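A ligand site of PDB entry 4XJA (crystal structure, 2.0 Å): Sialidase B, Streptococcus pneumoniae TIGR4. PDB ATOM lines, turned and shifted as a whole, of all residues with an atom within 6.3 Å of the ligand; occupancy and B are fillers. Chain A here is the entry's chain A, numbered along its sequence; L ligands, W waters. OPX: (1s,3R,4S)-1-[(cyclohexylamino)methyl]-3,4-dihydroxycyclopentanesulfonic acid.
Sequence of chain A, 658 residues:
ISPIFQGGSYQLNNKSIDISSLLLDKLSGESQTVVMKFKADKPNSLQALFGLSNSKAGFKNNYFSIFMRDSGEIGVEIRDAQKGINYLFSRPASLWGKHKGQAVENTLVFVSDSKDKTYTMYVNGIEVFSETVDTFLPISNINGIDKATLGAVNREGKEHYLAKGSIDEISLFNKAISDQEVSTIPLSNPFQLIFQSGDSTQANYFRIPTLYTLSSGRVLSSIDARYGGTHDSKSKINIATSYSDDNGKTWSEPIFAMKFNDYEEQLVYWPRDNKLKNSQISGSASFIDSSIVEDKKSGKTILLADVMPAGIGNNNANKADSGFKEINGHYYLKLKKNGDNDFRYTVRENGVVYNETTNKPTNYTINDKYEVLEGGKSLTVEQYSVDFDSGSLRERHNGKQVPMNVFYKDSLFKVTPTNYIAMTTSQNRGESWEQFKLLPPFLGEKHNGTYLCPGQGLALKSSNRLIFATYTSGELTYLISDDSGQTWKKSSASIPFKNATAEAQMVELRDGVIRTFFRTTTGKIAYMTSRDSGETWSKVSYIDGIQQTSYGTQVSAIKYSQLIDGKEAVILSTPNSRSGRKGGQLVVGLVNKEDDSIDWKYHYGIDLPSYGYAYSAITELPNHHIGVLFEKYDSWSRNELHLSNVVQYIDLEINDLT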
ATOM      1  N   LEU A 211       4.085  -0.126 -19.557  1.00  0.00           N
ATOM      2  CA  LEU A 211       3.424  -1.407 -19.798  1.00  0.00           C
ATOM      3  C   LEU A 211       2.166  -1.128 -20.596  1.00  0.00           C
ATOM      4  O   LEU A 211       1.513  -0.124 -20.369  1.00  0.00           O
ATOM      5  CB  LEU A 211       2.992  -2.072 -18.482  1.00  0.00           C
ATOM      6  CG  LEU A 211       4.043  -2.683 -17.576  1.00  0.00           C
ATOM      7  CD1 LEU A 211       3.394  -3.074 -16.237  1.00  0.00           C
ATOM      8  CD2 LEU A 211       4.660  -3.917 -18.249  1.00  0.00           C
ATOM      9  N   TYR A 212       1.809  -2.028 -21.518  1.00  0.00           N
ATOM     10  CA  TYR A 212       0.602  -1.839 -22.310  1.00  0.00           C
ATOM     11  C   TYR A 212       0.084  -3.217 -22.707  1.00  0.00           C
ATOM     12  O   TYR A 212       0.854  -4.073 -23.144  1.00  0.00           O
ATOM     13  CB  TYR A 212       0.916  -0.981 -23.544  1.00  0.00           C
ATOM     14  CG  TYR A 212      -0.323  -0.481 -24.287  1.00  0.00           C
ATOM     15  CD1 TYR A 212      -1.036  -1.304 -25.148  1.00  0.00           C
ATOM     16  CD2 TYR A 212      -0.772   0.831 -24.124  1.00  0.00           C
ATOM     17  CE1 TYR A 212      -2.156  -0.842 -25.833  1.00  0.00           C
ATOM     18  CE2 TYR A 212      -1.895   1.306 -24.809  1.00  0.00           C
ATOM     19  CZ  TYR A 212      -2.574   0.461 -25.661  1.00  0.00           C
ATOM     20  OH  TYR A 212      -3.695   0.923 -26.346  1.00  0.00           O
ATOM     21  N   THR A 213      -1.213  -3.447 -22.542  1.00  0.00           N
ATOM     22  CA  THR A 213      -1.764  -4.756 -22.884  1.00  0.00           C
ATOM     23  C   THR A 213      -2.352  -4.694 -24.293  1.00  0.00           C
ATOM     24  O   THR A 213      -3.297  -3.939 -24.537  1.00  0.00           O
ATOM     25  CB  THR A 213      -2.862  -5.168 -21.918  1.00  0.00           C
ATOM     26  OG1 THR A 213      -2.340  -5.134 -20.577  1.00  0.00           O
ATOM     27  CG2 THR A 213      -3.367  -6.576 -22.235  1.00  0.00           C
ATOM     28  N   LEU A 214      -1.791  -5.502 -25.194  1.00  0.00           N
ATOM     29  CA  LEU A 214      -2.221  -5.533 -26.591  1.00  0.00           C
ATOM     30  C   LEU A 214      -3.463  -6.441 -26.801  1.00  0.00           C
ATOM     31  O   LEU A 214      -3.767  -7.309 -25.976  1.00  0.00           O
ATOM     32  CB  LEU A 214      -1.062  -6.013 -27.473  1.00  0.00           C
ATOM     33  CG  LEU A 214       0.286  -5.302 -27.330  1.00  0.00           C
ATOM     34  CD1 LEU A 214       1.333  -5.925 -28.244  1.00  0.00           C
ATOM     35  CD2 LEU A 214       0.134  -3.805 -27.601  1.00  0.00           C
ATOM     36  N   LYS A 296      -6.199   0.228 -33.516  1.00  0.00           N
ATOM     37  CA  LYS A 296      -7.203  -0.720 -33.988  1.00  0.00           C
ATOM     38  C   LYS A 296      -7.201  -0.851 -35.507  1.00  0.00           C
ATOM     39  O   LYS A 296      -7.237  -1.959 -36.056  1.00  0.00           O
ATOM     40  CB  LYS A 296      -8.616  -0.283 -33.549  1.00  0.00           C
ATOM     41  CG  LYS A 296      -8.982  -0.436 -32.073  1.00  0.00           C
ATOM     42  CD  LYS A 296      -9.761   0.817 -31.601  1.00  0.00           C
ATOM     43  CE  LYS A 296     -10.831   0.533 -30.557  1.00  0.00           C
ATOM     44  NZ  LYS A 296     -10.304   0.173 -29.189  1.00  0.00           N
ATOM     45  N   GLN A 456       1.532   5.224 -21.281  1.00  0.00           N
ATOM     46  CA  GLN A 456       0.665   4.750 -22.336  1.00  0.00           C
ATOM     47  C   GLN A 456       0.084   5.930 -23.086  1.00  0.00           C
ATOM     48  O   GLN A 456      -0.167   6.987 -22.504  1.00  0.00           O
ATOM     49  CB  GLN A 456      -0.482   3.941 -21.736  1.00  0.00           C
ATOM     50  CG  GLN A 456      -0.070   2.906 -20.722  1.00  0.00           C
ATOM     51  CD  GLN A 456      -1.251   2.091 -20.214  1.00  0.00           C
ATOM     52  OE1 GLN A 456      -2.410   2.533 -20.312  1.00  0.00           O
ATOM     53  NE2 GLN A 456      -0.980   0.903 -19.672  1.00  0.00           N
ATOM     54  N   GLY A 457      -0.120   5.753 -24.391  1.00  0.00           N
ATOM     55  CA  GLY A 457      -1.012   6.636 -25.120  1.00  0.00           C
ATOM     56  C   GLY A 457      -2.401   6.061 -24.914  1.00  0.00           C
ATOM     57  O   GLY A 457      -2.552   5.048 -24.236  1.00  0.00           O
ATOM     58  N   LEU A 458      -3.413   6.704 -25.484  1.00  0.00           N
ATOM     59  CA  LEU A 458      -4.784   6.250 -25.286  1.00  0.00           C
ATOM     60  C   LEU A 458      -5.445   5.948 -26.618  1.00  0.00           C
ATOM     61  O   LEU A 458      -5.424   6.765 -27.537  1.00  0.00           O
ATOM     62  CB  LEU A 458      -5.596   7.310 -24.550  1.00  0.00           C
ATOM     63  CG  LEU A 458      -7.104   7.072 -24.397  1.00  0.00           C
ATOM     64  CD1 LEU A 458      -7.364   5.967 -23.399  1.00  0.00           C
ATOM     65  CD2 LEU A 458      -7.789   8.364 -23.959  1.00  0.00           C
ATOM     66  N   ALA A 459      -6.008   4.744 -26.726  1.00  0.00           N
ATOM     67  CA  ALA A 459      -6.836   4.386 -27.879  1.00  0.00           C
ATOM     68  C   ALA A 459      -8.293   4.410 -27.430  1.00  0.00           C
ATOM     69  O   ALA A 459      -8.654   3.692 -26.497  1.00  0.00           O
ATOM     70  CB  ALA A 459      -6.466   2.989 -28.383  1.00  0.00           C
ATOM     71  N   LYS A 461     -12.294   3.740 -27.196  1.00  0.00           N
ATOM     72  CA  LYS A 461     -13.067   2.503 -27.425  1.00  0.00           C
ATOM     73  C   LYS A 461     -13.829   2.518 -28.749  1.00  0.00           C
ATOM     74  O   LYS A 461     -13.827   1.530 -29.486  1.00  0.00           O
ATOM     75  CB  LYS A 461     -14.095   2.269 -26.309  1.00  0.00           C
ATOM     76  CG  LYS A 461     -13.592   2.455 -24.871  1.00  0.00           C
ATOM     77  CD  LYS A 461     -14.778   2.421 -23.884  1.00  0.00           C
ATOM     78  CE  LYS A 461     -14.509   3.257 -22.619  1.00  0.00           C
ATOM     79  NZ  LYS A 461     -13.447   2.678 -21.735  1.00  0.00           N
ATOM     80  N   ALA A 557      -2.008   5.388 -14.552  1.00  0.00           N
ATOM     81  CA  ALA A 557      -3.460   5.293 -14.347  1.00  0.00           C
ATOM     82  C   ALA A 557      -4.119   4.374 -15.382  1.00  0.00           C
ATOM     83  O   ALA A 557      -3.837   4.486 -16.559  1.00  0.00           O
ATOM     84  CB  ALA A 557      -4.083   6.680 -14.407  1.00  0.00           C
ATOM     85  N   ILE A 558      -5.020   3.507 -14.938  1.00  0.00           N
ATOM     86  CA  ILE A 558      -5.776   2.684 -15.871  1.00  0.00           C
ATOM     87  C   ILE A 558      -7.236   2.637 -15.467  1.00  0.00           C
ATOM     88  O   ILE A 558      -7.581   2.897 -14.318  1.00  0.00           O
ATOM     89  CB  ILE A 558      -5.254   1.233 -15.919  1.00  0.00           C
ATOM     90  CG1 ILE A 558      -5.310   0.614 -14.528  1.00  0.00           C
ATOM     91  CG2 ILE A 558      -3.845   1.181 -16.516  1.00  0.00           C
ATOM     92  CD1 ILE A 558      -5.019  -0.890 -14.499  1.00  0.00           C
ATOM     93  N   LYS A 559      -8.087   2.324 -16.447  1.00  0.00           N
ATOM     94  CA  LYS A 559      -9.469   2.017 -16.172  1.00  0.00           C
ATOM     95  C   LYS A 559      -9.586   0.493 -16.132  1.00  0.00           C
ATOM     96  O   LYS A 559      -9.276  -0.183 -17.123  1.00  0.00           O
ATOM     97  CB  LYS A 559     -10.350   2.586 -17.303  1.00  0.00           C
ATOM     98  CG  LYS A 559     -11.813   2.187 -17.231  1.00  0.00           C
ATOM     99  CD  LYS A 559     -12.531   2.949 -16.154  1.00  0.00           C
ATOM    100  CE  LYS A 559     -13.982   2.494 -16.059  1.00  0.00           C
ATOM    101  NZ  LYS A 559     -14.625   2.488 -17.398  1.00  0.00           N
ATOM    102  N   SER A 561     -11.182  -3.170 -16.301  1.00  0.00           N
ATOM    103  CA  SER A 561     -12.265  -3.647 -17.164  1.00  0.00           C
ATOM    104  C   SER A 561     -13.450  -4.233 -16.385  1.00  0.00           C
ATOM    105  O   SER A 561     -14.543  -4.368 -16.931  1.00  0.00           O
ATOM    106  CB  SER A 561     -11.762  -4.706 -18.145  1.00  0.00           C
ATOM    107  OG  SER A 561     -11.575  -5.935 -17.471  1.00  0.00           O
ATOM    108  N   ILE A 618       1.478   0.618 -14.909  1.00  0.00           N
ATOM    109  CA  ILE A 618       0.525  -0.411 -14.530  1.00  0.00           C
ATOM    110  C   ILE A 618      -0.324  -0.795 -15.706  1.00  0.00           C
ATOM    111  O   ILE A 618      -0.634   0.040 -16.570  1.00  0.00           O
ATOM    112  CB  ILE A 618      -0.386   0.016 -13.373  1.00  0.00           C
ATOM    113  CG1 ILE A 618      -1.057   1.336 -13.682  1.00  0.00           C
ATOM    114  CG2 ILE A 618       0.409   0.111 -12.049  1.00  0.00           C
ATOM    115  CD1 ILE A 618      -1.992   1.760 -12.584  1.00  0.00           C
ATOM    116  N   THR A 619      -0.732  -2.052 -15.742  1.00  0.00           N
ATOM    117  CA  THR A 619      -1.626  -2.460 -16.803  1.00  0.00           C
ATOM    118  C   THR A 619      -2.455  -3.629 -16.348  1.00  0.00           C
ATOM    119  O   THR A 619      -2.012  -4.417 -15.497  1.00  0.00           O
ATOM    120  CB  THR A 619      -0.863  -2.740 -18.133  1.00  0.00           C
ATOM    121  OG1 THR A 619      -1.782  -2.664 -19.229  1.00  0.00           O
ATOM    122  CG2 THR A 619      -0.190  -4.121 -18.122  1.00  0.00           C
ATOM    123  N   GLU A 620      -3.686  -3.706 -16.845  1.00  0.00           N
ATOM    124  CA  GLU A 620      -4.503  -4.865 -16.585  1.00  0.00           C
ATOM    125  C   GLU A 620      -4.052  -5.998 -17.507  1.00  0.00           C
ATOM    126  O   GLU A 620      -4.039  -5.869 -18.736  1.00  0.00           O
ATOM    127  CB  GLU A 620      -6.008  -4.562 -16.794  1.00  0.00           C
ATOM    128  CG  GLU A 620      -6.899  -5.757 -16.458  1.00  0.00           C
ATOM    129  CD  GLU A 620      -8.378  -5.452 -16.544  1.00  0.00           C
ATOM    130  OE1 GLU A 620      -8.734  -4.263 -16.751  1.00  0.00           O
ATOM    131  OE2 GLU A 620      -9.191  -6.394 -16.397  1.00  0.00           O
ATOM    132  N   LEU A 621      -3.650  -7.113 -16.895  1.00  0.00           N
ATOM    133  CA  LEU A 621      -3.189  -8.256 -17.683  1.00  0.00           C
ATOM    134  C   LEU A 621      -4.434  -8.924 -18.227  1.00  0.00           C
ATOM    135  O   LEU A 621      -5.537  -8.677 -17.731  1.00  0.00           O
ATOM    136  CB  LEU A 621      -2.365  -9.199 -16.802  1.00  0.00           C
ATOM    137  CG  LEU A 621      -1.156  -8.515 -16.152  1.00  0.00           C
ATOM    138  CD1 LEU A 621      -0.585  -9.334 -15.013  1.00  0.00           C
ATOM    139  CD2 LEU A 621      -0.076  -8.228 -17.188  1.00  0.00           C
ATOM    140  N   PRO A 622      -4.282  -9.738 -19.285  1.00  0.00           N
ATOM    141  CA  PRO A 622      -5.472 -10.347 -19.888  1.00  0.00           C
ATOM    142  C   PRO A 622      -6.278 -11.248 -18.937  1.00  0.00           C
ATOM    143  O   PRO A 622      -7.467 -11.470 -19.202  1.00  0.00           O
ATOM    144  CB  PRO A 622      -4.892 -11.183 -21.028  1.00  0.00           C
ATOM    145  CG  PRO A 622      -3.641 -10.445 -21.421  1.00  0.00           C
ATOM    146  CD  PRO A 622      -3.084  -9.955 -20.113  1.00  0.00           C
ATOM    147  N   ASN A 623      -5.646 -11.751 -17.870  1.00  0.00           N
ATOM    148  CA  ASN A 623      -6.351 -12.584 -16.900  1.00  0.00           C
ATOM    149  C   ASN A 623      -6.971 -11.779 -15.761  1.00  0.00           C
ATOM    150  O   ASN A 623      -7.396 -12.335 -14.737  1.00  0.00           O
ATOM    151  CB  ASN A 623      -5.416 -13.647 -16.322  1.00  0.00           C
ATOM    152  CG  ASN A 623      -4.214 -13.047 -15.633  1.00  0.00           C
ATOM    153  OD1 ASN A 623      -4.082 -11.823 -15.538  1.00  0.00           O
ATOM    154  ND2 ASN A 623      -3.317 -13.904 -15.140  1.00  0.00           N
ATOM    155  N   HIS A 624      -6.980 -10.455 -15.935  1.00  0.00           N
ATOM    156  CA  HIS A 624      -7.520  -9.485 -14.966  1.00  0.00           C
ATOM    157  C   HIS A 624      -6.681  -9.260 -13.705  1.00  0.00           C
ATOM    158  O   HIS A 624      -7.125  -8.570 -12.779  1.00  0.00           O
ATOM    159  CB  HIS A 624      -8.986  -9.777 -14.650  1.00  0.00           C
ATOM    160  CG  HIS A 624      -9.836  -9.876 -15.863  1.00  0.00           C
ATOM    161  ND1 HIS A 624      -9.941  -8.835 -16.788  1.00  0.00           N
ATOM    162  CD2 HIS A 624     -10.598 -10.879 -16.364  1.00  0.00           C
ATOM    163  CE1 HIS A 624     -10.722  -9.196 -17.762  1.00  0.00           C
ATOM    164  NE2 HIS A 624     -11.144 -10.445 -17.549  1.00  0.00           N
HETATM  165  CAF OPX L   1      -8.250  -7.074 -20.169  1.00  0.00           C
HETATM  166  CAG OPX L   1      -9.136  -6.704 -21.299  1.00  0.00           C
HETATM  167  CAH OPX L   1      -6.850  -6.582 -20.411  1.00  0.00           C
HETATM  168  CAI OPX L   1      -9.027  -5.253 -21.713  1.00  0.00           C
HETATM  169  CAJ OPX L   1      -6.832  -5.102 -20.657  1.00  0.00           C
HETATM  170  CAK OPX L   1      -6.276  -2.822 -22.569  1.00  0.00           C
HETATM  171  CAL OPX L   1      -6.001  -0.630 -21.316  1.00  0.00           C
HETATM  172  CAM OPX L   1      -4.773  -1.023 -23.316  1.00  0.00           C
HETATM  173  CAO OPX L   1      -4.780   0.248 -21.375  1.00  0.00           C
HETATM  174  CAP OPX L   1      -3.884  -0.458 -22.221  1.00  0.00           C
HETATM  175  CAQ OPX L   1      -7.608  -4.767 -21.877  1.00  0.00           C
HETATM  176  CAR OPX L   1      -6.073  -1.297 -22.657  1.00  0.00           C
HETATM  177  NAN OPX L   1      -7.591  -3.305 -22.050  1.00  0.00           N
HETATM  178  OAA OPX L   1      -8.660  -0.744 -22.976  1.00  0.00           O
HETATM  179  OAB OPX L   1      -7.111   1.021 -23.681  1.00  0.00           O
HETATM  180  OAC OPX L   1      -4.256   0.301 -20.107  1.00  0.00           O
HETATM  181  OAD OPX L   1      -3.392  -1.547 -21.533  1.00  0.00           O
HETATM  182  OAE OPX L   1      -7.363  -1.017 -25.022  1.00  0.00           O
HETATM  183  SAS OPX L   1      -7.350  -0.468 -23.626  1.00  0.00           S
HETATM  184  O   HOH W   1      -5.036  -1.640 -18.214  1.00  0.00           O
HETATM  185  O   HOH W   2      -6.904   2.037 -18.989  1.00  0.00           O
HETATM  186  O   HOH W   3      -9.131  -3.200 -24.498  1.00  0.00           O
HETATM  187  O   HOH W   4      -9.661   3.312 -24.065  1.00  0.00           O
HETATM  188  O   HOH W   5      -5.450  -0.790 -27.035  1.00  0.00           O
HETATM  189  O   HOH W   6      -5.282   2.651 -24.897  1.00  0.00           O
HETATM  190  O   HOH W   7      -9.404   0.831 -20.288  1.00  0.00           O
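The backbone NH of Thr 213 is in hydrogen-bond range of an oxygen (OAD) of the ligand (3.1 Å).
OG1 of Thr 619 is in hydrogen-bond range of OAD of the ligand, at 3.0 Å.
The side-chain amide oxygen of Gln 456 is in hydrogen-bond range of an oxygen (OAC) of the ligand (2.9 Å).
NE2 of Gln 456 lies within hydrogen-bond range of O of Leu 211, at 2.8 Å.
OE2 of Glu 620 lies within hydrogen-bond range of OG of Ser 561 (2.7 Å).
O of Glu 620 is in hydrogen-bond range of OG1 of Thr 213, at 2.6 Å.
The side-chain amide nitrogen (NE2) of Gln 456 lies within hydrogen-bond range of the backbone carbonyl oxygen (O) of Ile 618 (3.2 Å).
The side-chain hydroxyl (OG1) of Thr 619 sits at hydrogen-bond distance from the side-chain hydroxyl (OG1) of Thr 213, 2.9 Å away.
The side-chain carboxylate of Glu 620 sits at hydrogen-bond distance from a ring nitrogen (ND1) of His 624 (2.6 Å).
CZ of Tyr 212 touches CAM of the ligand, 3.5 Å away.
CG2 of Ile 558 touches OAC of the ligand, 3.7 Å away.
Glu 620 touches the ligand (O to CAH, 3.3 Å).
Leu 621 touches the ligand.
Of the 21 residues printed, 7 come within 4 Å of the ligand.
Water W6 lies within hydrogen-bond range of an oxygen (OAB) of the ligand (2.7 Å), the side-chain hydroxyl of Tyr 212 (2.8 Å) and the backbone NH of Ala 459 (2.9 Å).
Water W5 lies within hydrogen-bond range of OH of Tyr 212 (2.5 Å) and OAE of the ligand (2.8 Å).
Water W1 lies within hydrogen-bond range of OAC of the ligand (2.8 Å) and N of Glu 620 (2.8 Å).
Water W7 bridges an oxygen (OAA) of the ligand (3.2 Å) and the backbone carbonyl oxygen (O) of Lys 559 (3.3 Å).
Water W2 lies within hydrogen-bond range of the backbone NH (N) of Lys 559 (2.8 Å) and an oxygen (OAC) of the ligand (3.4 Å).
Water W4 lies within hydrogen-bond range of O of Ala 459 (2.7 Å) and OAB of the ligand (3.4 Å).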
